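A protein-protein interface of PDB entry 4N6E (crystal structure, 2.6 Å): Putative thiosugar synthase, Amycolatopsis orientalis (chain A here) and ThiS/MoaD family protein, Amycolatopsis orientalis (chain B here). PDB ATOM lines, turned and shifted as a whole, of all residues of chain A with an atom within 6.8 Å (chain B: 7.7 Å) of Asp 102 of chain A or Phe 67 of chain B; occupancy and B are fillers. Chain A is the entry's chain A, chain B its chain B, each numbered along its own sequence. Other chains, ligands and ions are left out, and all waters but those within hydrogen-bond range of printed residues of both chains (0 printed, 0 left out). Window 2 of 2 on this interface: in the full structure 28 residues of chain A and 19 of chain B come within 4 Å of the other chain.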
ATOM      1  N   ALA A  97     -12.074 -35.276  -6.060  1.00  0.00           N
ATOM      2  CA  ALA A  97     -12.690 -34.422  -5.029  1.00  0.00           C
ATOM      3  C   ALA A  97     -11.715 -33.349  -4.512  1.00  0.00           C
ATOM      4  O   ALA A  97     -12.077 -32.184  -4.341  1.00  0.00           O
ATOM      5  CB  ALA A  97     -13.217 -35.256  -3.871  1.00  0.00           C
ATOM      6  N   ARG A  98     -10.473 -33.750  -4.279  1.00  0.00           N
ATOM      7  CA  ARG A  98      -9.464 -32.819  -3.775  1.00  0.00           C
ATOM      8  C   ARG A  98      -8.909 -31.893  -4.855  1.00  0.00           C
ATOM      9  O   ARG A  98      -8.391 -30.831  -4.544  1.00  0.00           O
ATOM     10  CB  ARG A  98      -8.343 -33.593  -3.097  1.00  0.00           C
ATOM     11  CG  ARG A  98      -8.852 -34.313  -1.878  1.00  0.00           C
ATOM     12  CD  ARG A  98      -7.849 -35.241  -1.252  1.00  0.00           C
ATOM     13  NE  ARG A  98      -8.418 -35.673   0.024  1.00  0.00           N
ATOM     14  CZ  ARG A  98      -8.542 -36.927   0.454  1.00  0.00           C
ATOM     15  NH1 ARG A  98      -8.088 -37.945  -0.249  1.00  0.00           N
ATOM     16  NH2 ARG A  98      -9.127 -37.149   1.633  1.00  0.00           N
ATOM     17  N   ILE A  99      -9.013 -32.284  -6.119  1.00  0.00           N
ATOM     18  CA  ILE A  99      -8.661 -31.366  -7.197  1.00  0.00           C
ATOM     19  C   ILE A  99      -9.742 -30.285  -7.332  1.00  0.00           C
ATOM     20  O   ILE A  99      -9.436 -29.109  -7.594  1.00  0.00           O
ATOM     21  CB  ILE A  99      -8.487 -32.096  -8.526  1.00  0.00           C
ATOM     22  CG1 ILE A  99      -7.184 -32.872  -8.516  1.00  0.00           C
ATOM     23  CG2 ILE A  99      -8.512 -31.115  -9.686  1.00  0.00           C
ATOM     24  CD1 ILE A  99      -7.063 -33.861  -9.657  1.00  0.00           C
ATOM     25  N   LEU A 100     -10.998 -30.678  -7.144  1.00  0.00           N
ATOM     26  CA  LEU A 100     -12.101 -29.721  -7.239  1.00  0.00           C
ATOM     27  C   LEU A 100     -12.071 -28.721  -6.104  1.00  0.00           C
ATOM     28  O   LEU A 100     -12.416 -27.553  -6.288  1.00  0.00           O
ATOM     29  CB  LEU A 100     -13.452 -30.439  -7.294  1.00  0.00           C
ATOM     30  CG  LEU A 100     -13.649 -31.246  -8.576  1.00  0.00           C
ATOM     31  CD1 LEU A 100     -14.779 -32.249  -8.432  1.00  0.00           C
ATOM     32  CD2 LEU A 100     -13.900 -30.316  -9.757  1.00  0.00           C
ATOM     33  N   ARG A 101     -11.646 -29.169  -4.932  1.00  0.00           N
ATOM     34  CA  ARG A 101     -11.497 -28.274  -3.798  1.00  0.00           C
ATOM     35  C   ARG A 101     -10.411 -27.244  -4.079  1.00  0.00           C
ATOM     36  O   ARG A 101     -10.649 -26.046  -4.007  1.00  0.00           O
ATOM     37  CB  ARG A 101     -11.143 -29.060  -2.551  1.00  0.00           C
ATOM     38  CG  ARG A 101     -10.927 -28.201  -1.317  1.00  0.00           C
ATOM     39  CD  ARG A 101     -10.170 -28.988  -0.278  1.00  0.00           C
ATOM     40  NE  ARG A 101      -8.909 -29.474  -0.824  1.00  0.00           N
ATOM     41  CZ  ARG A 101      -8.215 -30.500  -0.339  1.00  0.00           C
ATOM     42  NH1 ARG A 101      -8.658 -31.172   0.713  1.00  0.00           N
ATOM     43  NH2 ARG A 101      -7.059 -30.860  -0.912  1.00  0.00           N
ATOM     44  N   ASP A 102      -9.224 -27.723  -4.409  1.00  0.00           N
ATOM     45  CA  ASP A 102      -8.070 -26.842  -4.607  1.00  0.00           C
ATOM     46  C   ASP A 102      -8.247 -25.859  -5.779  1.00  0.00           C
ATOM     47  O   ASP A 102      -7.929 -24.677  -5.660  1.00  0.00           O
ATOM     48  CB  ASP A 102      -6.801 -27.691  -4.781  1.00  0.00           C
ATOM     49  CG  ASP A 102      -6.466 -28.499  -3.527  1.00  0.00           C
ATOM     50  OD1 ASP A 102      -6.960 -28.144  -2.432  1.00  0.00           O
ATOM     51  OD2 ASP A 102      -5.717 -29.498  -3.624  1.00  0.00           O
ATOM     52  N   SER A 103      -8.778 -26.350  -6.889  1.00  0.00           N
ATOM     53  CA  SER A 103      -8.852 -25.576  -8.123  1.00  0.00           C
ATOM     54  C   SER A 103     -10.028 -24.577  -8.201  1.00  0.00           C
ATOM     55  O   SER A 103      -9.899 -23.513  -8.809  1.00  0.00           O
ATOM     56  CB  SER A 103      -8.939 -26.540  -9.308  1.00  0.00           C
ATOM     57  OG  SER A 103     -10.136 -27.307  -9.251  1.00  0.00           O
ATOM     58  N   LEU A 104     -11.172 -24.935  -7.623  1.00  0.00           N
ATOM     59  CA  LEU A 104     -12.392 -24.110  -7.706  1.00  0.00           C
ATOM     60  C   LEU A 104     -12.950 -23.720  -6.355  1.00  0.00           C
ATOM     61  O   LEU A 104     -13.915 -22.965  -6.296  1.00  0.00           O
ATOM     62  CB  LEU A 104     -13.498 -24.834  -8.496  1.00  0.00           C
ATOM     63  CG  LEU A 104     -13.142 -25.315  -9.905  1.00  0.00           C
ATOM     64  CD1 LEU A 104     -14.304 -26.043 -10.568  1.00  0.00           C
ATOM     65  CD2 LEU A 104     -12.703 -24.138 -10.748  1.00  0.00           C
ATOM     66  N   GLY A 105     -12.359 -24.219  -5.274  1.00  0.00           N
ATOM     67  CA  GLY A 105     -12.856 -23.913  -3.931  1.00  0.00           C
ATOM     68  C   GLY A 105     -14.178 -24.596  -3.610  1.00  0.00           C
ATOM     69  O   GLY A 105     -14.883 -24.171  -2.699  1.00  0.00           O
ATOM     70  N   ILE A 106     -14.501 -25.664  -4.348  1.00  0.00           N
ATOM     71  CA  ILE A 106     -15.694 -26.466  -4.100  1.00  0.00           C
ATOM     72  C   ILE A 106     -15.730 -26.968  -2.651  1.00  0.00           C
ATOM     73  O   ILE A 106     -14.810 -27.643  -2.201  1.00  0.00           O
ATOM     74  CB  ILE A 106     -15.756 -27.683  -5.057  1.00  0.00           C
ATOM     75  CG1 ILE A 106     -16.014 -27.239  -6.498  1.00  0.00           C
ATOM     76  CG2 ILE A 106     -16.833 -28.677  -4.653  1.00  0.00           C
ATOM     77  CD1 ILE A 106     -17.386 -26.667  -6.762  1.00  0.00           C
ATOM     78  N   ASN B  57      -6.373 -26.682 -15.221  1.00  0.00           N
ATOM     79  CA  ASN B  57      -5.377 -27.185 -14.286  1.00  0.00           C
ATOM     80  C   ASN B  57      -4.239 -27.815 -15.042  1.00  0.00           C
ATOM     81  O   ASN B  57      -4.459 -28.516 -16.030  1.00  0.00           O
ATOM     82  CB  ASN B  57      -5.979 -28.232 -13.359  1.00  0.00           C
ATOM     83  CG  ASN B  57      -7.286 -27.784 -12.766  1.00  0.00           C
ATOM     84  OD1 ASN B  57      -7.316 -26.869 -11.946  1.00  0.00           O
ATOM     85  ND2 ASN B  57      -8.383 -28.409 -13.194  1.00  0.00           N
ATOM     86  N   VAL B  58      -3.018 -27.574 -14.575  1.00  0.00           N
ATOM     87  CA  VAL B  58      -1.843 -28.201 -15.166  1.00  0.00           C
ATOM     88  C   VAL B  58      -1.046 -28.944 -14.109  1.00  0.00           C
ATOM     89  O   VAL B  58      -0.741 -28.394 -13.067  1.00  0.00           O
ATOM     90  CB  VAL B  58      -0.930 -27.166 -15.837  1.00  0.00           C
ATOM     91  CG1 VAL B  58       0.350 -27.830 -16.324  1.00  0.00           C
ATOM     92  CG2 VAL B  58      -1.662 -26.470 -16.983  1.00  0.00           C
ATOM     93  N   TYR B  59      -0.701 -30.192 -14.400  1.00  0.00           N
ATOM     94  CA  TYR B  59       0.107 -30.999 -13.505  1.00  0.00           C
ATOM     95  C   TYR B  59       1.460 -31.333 -14.129  1.00  0.00           C
ATOM     96  O   TYR B  59       1.557 -31.542 -15.348  1.00  0.00           O
ATOM     97  CB  TYR B  59      -0.643 -32.274 -13.135  1.00  0.00           C
ATOM     98  CG  TYR B  59      -1.957 -31.973 -12.474  1.00  0.00           C
ATOM     99  CD1 TYR B  59      -3.096 -31.698 -13.238  1.00  0.00           C
ATOM    100  CD2 TYR B  59      -2.069 -31.939 -11.092  1.00  0.00           C
ATOM    101  CE1 TYR B  59      -4.306 -31.398 -12.635  1.00  0.00           C
ATOM    102  CE2 TYR B  59      -3.274 -31.643 -10.479  1.00  0.00           C
ATOM    103  CZ  TYR B  59      -4.386 -31.372 -11.257  1.00  0.00           C
ATOM    104  OH  TYR B  59      -5.581 -31.080 -10.658  1.00  0.00           O
ATOM    105  N   GLU B  63       1.675 -33.447 -10.022  1.00  0.00           N
ATOM    106  CA  GLU B  63       1.666 -32.412  -8.982  1.00  0.00           C
ATOM    107  C   GLU B  63       1.081 -31.124  -9.541  1.00  0.00           C
ATOM    108  O   GLU B  63       1.568 -30.605 -10.537  1.00  0.00           O
ATOM    109  CB  GLU B  63       3.083 -32.129  -8.465  1.00  0.00           C
ATOM    110  CG  GLU B  63       3.645 -33.160  -7.490  1.00  0.00           C
ATOM    111  CD  GLU B  63       5.011 -32.753  -6.928  1.00  0.00           C
ATOM    112  OE1 GLU B  63       5.163 -31.576  -6.506  1.00  0.00           O
ATOM    113  OE2 GLU B  63       5.938 -33.606  -6.905  1.00  0.00           O
ATOM    114  N   ASP B  64       0.052 -30.599  -8.885  1.00  0.00           N
ATOM    115  CA  ASP B  64      -0.597 -29.364  -9.326  1.00  0.00           C
ATOM    116  C   ASP B  64       0.387 -28.202  -9.255  1.00  0.00           C
ATOM    117  O   ASP B  64       0.900 -27.870  -8.176  1.00  0.00           O
ATOM    118  CB  ASP B  64      -1.827 -29.071  -8.459  1.00  0.00           C
ATOM    119  CG  ASP B  64      -2.618 -27.852  -8.929  1.00  0.00           C
ATOM    120  OD1 ASP B  64      -2.060 -26.996  -9.649  1.00  0.00           O
ATOM    121  OD2 ASP B  64      -3.809 -27.748  -8.560  1.00  0.00           O
ATOM    122  N   VAL B  65       0.613 -27.572 -10.405  1.00  0.00           N
ATOM    123  CA  VAL B  65       1.595 -26.505 -10.526  1.00  0.00           C
ATOM    124  C   VAL B  65       1.286 -25.244  -9.745  1.00  0.00           C
ATOM    125  O   VAL B  65       2.199 -24.445  -9.518  1.00  0.00           O
ATOM    126  CB  VAL B  65       1.825 -26.075 -11.989  1.00  0.00           C
ATOM    127  CG1 VAL B  65       2.367 -27.239 -12.808  1.00  0.00           C
ATOM    128  CG2 VAL B  65       0.566 -25.469 -12.600  1.00  0.00           C
ATOM    129  N   ARG B  66       0.026 -25.038  -9.357  1.00  0.00           N
ATOM    130  CA  ARG B  66      -0.337 -23.856  -8.541  1.00  0.00           C
ATOM    131  C   ARG B  66       0.384 -23.844  -7.196  1.00  0.00           C
ATOM    132  O   ARG B  66       0.753 -22.785  -6.714  1.00  0.00           O
ATOM    133  CB  ARG B  66      -1.856 -23.755  -8.311  1.00  0.00           C
ATOM    134  CG  ARG B  66      -2.640 -23.133  -9.466  1.00  0.00           C
ATOM    135  CD  ARG B  66      -4.064 -22.778  -9.048  1.00  0.00           C
ATOM    136  NE  ARG B  66      -5.039 -23.289 -10.012  1.00  0.00           N
ATOM    137  CZ  ARG B  66      -5.518 -24.536 -10.037  1.00  0.00           C
ATOM    138  NH1 ARG B  66      -6.392 -24.872 -10.981  1.00  0.00           N
ATOM    139  NH2 ARG B  66      -5.139 -25.450  -9.136  1.00  0.00           N
ATOM    140  N   PHE B  67       0.603 -25.025  -6.615  1.00  0.00           N
ATOM    141  CA  PHE B  67       1.370 -25.159  -5.368  1.00  0.00           C
ATOM    142  C   PHE B  67       2.887 -25.060  -5.543  1.00  0.00           C
ATOM    143  O   PHE B  67       3.629 -25.265  -4.582  1.00  0.00           O
ATOM    144  CB  PHE B  67       1.067 -26.498  -4.682  1.00  0.00           C
ATOM    145  CG  PHE B  67      -0.369 -26.677  -4.297  1.00  0.00           C
ATOM    146  CD1 PHE B  67      -0.978 -25.790  -3.432  1.00  0.00           C
ATOM    147  CD2 PHE B  67      -1.102 -27.756  -4.784  1.00  0.00           C
ATOM    148  CE1 PHE B  67      -2.303 -25.955  -3.076  1.00  0.00           C
ATOM    149  CE2 PHE B  67      -2.429 -27.923  -4.435  1.00  0.00           C
ATOM    150  CZ  PHE B  67      -3.033 -27.019  -3.581  1.00  0.00           C
ATOM    151  N   SER B  68       3.346 -24.743  -6.750  1.00  0.00           N
ATOM    152  CA  SER B  68       4.759 -24.884  -7.102  1.00  0.00           C
ATOM    153  C   SER B  68       5.319 -23.820  -8.099  1.00  0.00           C
ATOM    154  O   SER B  68       6.401 -24.009  -8.648  1.00  0.00           O
ATOM    155  CB  SER B  68       4.944 -26.311  -7.635  1.00  0.00           C
ATOM    156  OG  SER B  68       6.198 -26.489  -8.248  1.00  0.00           O
ATOM    157  N   GLY B  69       4.603 -22.712  -8.318  1.00  0.00           N
ATOM    158  CA  GLY B  69       5.072 -21.637  -9.205  1.00  0.00           C
ATOM    159  C   GLY B  69       4.112 -21.174 -10.297  1.00  0.00           C
ATOM    160  O   GLY B  69       4.317 -20.114 -10.903  1.00  0.00           O
ATOM    161  N   GLY B  70       3.065 -21.961 -10.559  1.00  0.00           N
ATOM    162  CA  GLY B  70       2.146 -21.696 -11.671  1.00  0.00           C
ATOM    163  C   GLY B  70       2.830 -21.842 -13.028  1.00  0.00           C
ATOM    164  O   GLY B  70       3.429 -22.871 -13.333  1.00  0.00           O
ATOM    165  N   ALA B  73       6.625 -22.794 -12.790  1.00  0.00           N
ATOM    166  CA  ALA B  73       7.018 -24.045 -12.135  1.00  0.00           C
ATOM    167  C   ALA B  73       8.035 -24.818 -12.972  1.00  0.00           C
ATOM    168  O   ALA B  73       7.946 -24.828 -14.198  1.00  0.00           O
ATOM    169  CB  ALA B  73       5.796 -24.914 -11.857  1.00  0.00           C
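Among the printed residues, pairs that only touch across the chains: Ile 99 of chain A with Tyr 59 of chain B (3.1 Å), Ser 103 of chain A with Asn 57 of chain B (3.1 Å), Ser 103 of chain A with Arg 66 of chain B (3.5 Å) and Asp 102 of chain A with Phe 67 of chain B (3.7 Å).
The backbone carbonyl oxygen (O) of Ile 99 of chain A lies within hydrogen-bond range of the side-chain hydroxyl (OG) of Ser 103 of chain A (2.5 Å). The side-chain carboxylate (OD1) of Asp 102 of chain A lies within salt-bridge range of the guanidinium group (NE) of Arg 101 of chain A, at 2.9 Å. NH1 of Arg 66 of chain B lies within hydrogen-bond range of OD1 of Asn 57 of chain B (2.4 Å). NH2 of Arg 66 of chain B is in salt-bridge range of OD2 of Asp 64 of chain B (2.7 Å).
Of chain B, only Phe 67 comes within 4 Å of Asp 102 of chain A. Phe 67 of chain B touches one residue of chain A. Printed residues of chain A within 4 Å of Asn 57 of chain B: Ser 103. Of the printed residues of chain B, Ile 99 of chain A touches Tyr 59. Of the printed residues of chain A, Tyr 59 of chain B touches Ile 99. Of the printed residues of chain B, Ser 103 of chain A touches Asn 57 and Arg 66. Gly 69 of chain B touches none of the printed residues of chain A. The nearest residue of chain A that does not touch Phe 67 of chain B is Arg 101 of chain A (6.2 Å). The nearest printed residue of chain A that does not touch Arg 66 of chain B is Asp 102 of chain A (4.5 Å).
Of the 10 printed residues of chain A, 3 touch a printed residue of chain B. Hydrophobic or aromatic side chains of chain A that line the printed part of chain B: Ile 99. Printed residues of chain B that touch a printed residue of chain A: Asn 57, Tyr 59, Arg 66 and Phe 67. Hydrophobic or aromatic side chains of chain B within 4 Å of the printed part of chain A: Tyr 59 and Phe 67. Among the printed residues, no Asp or Glu carboxylate lies within 4 Å of a Lys or Arg side-chain nitrogen of the other chain.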
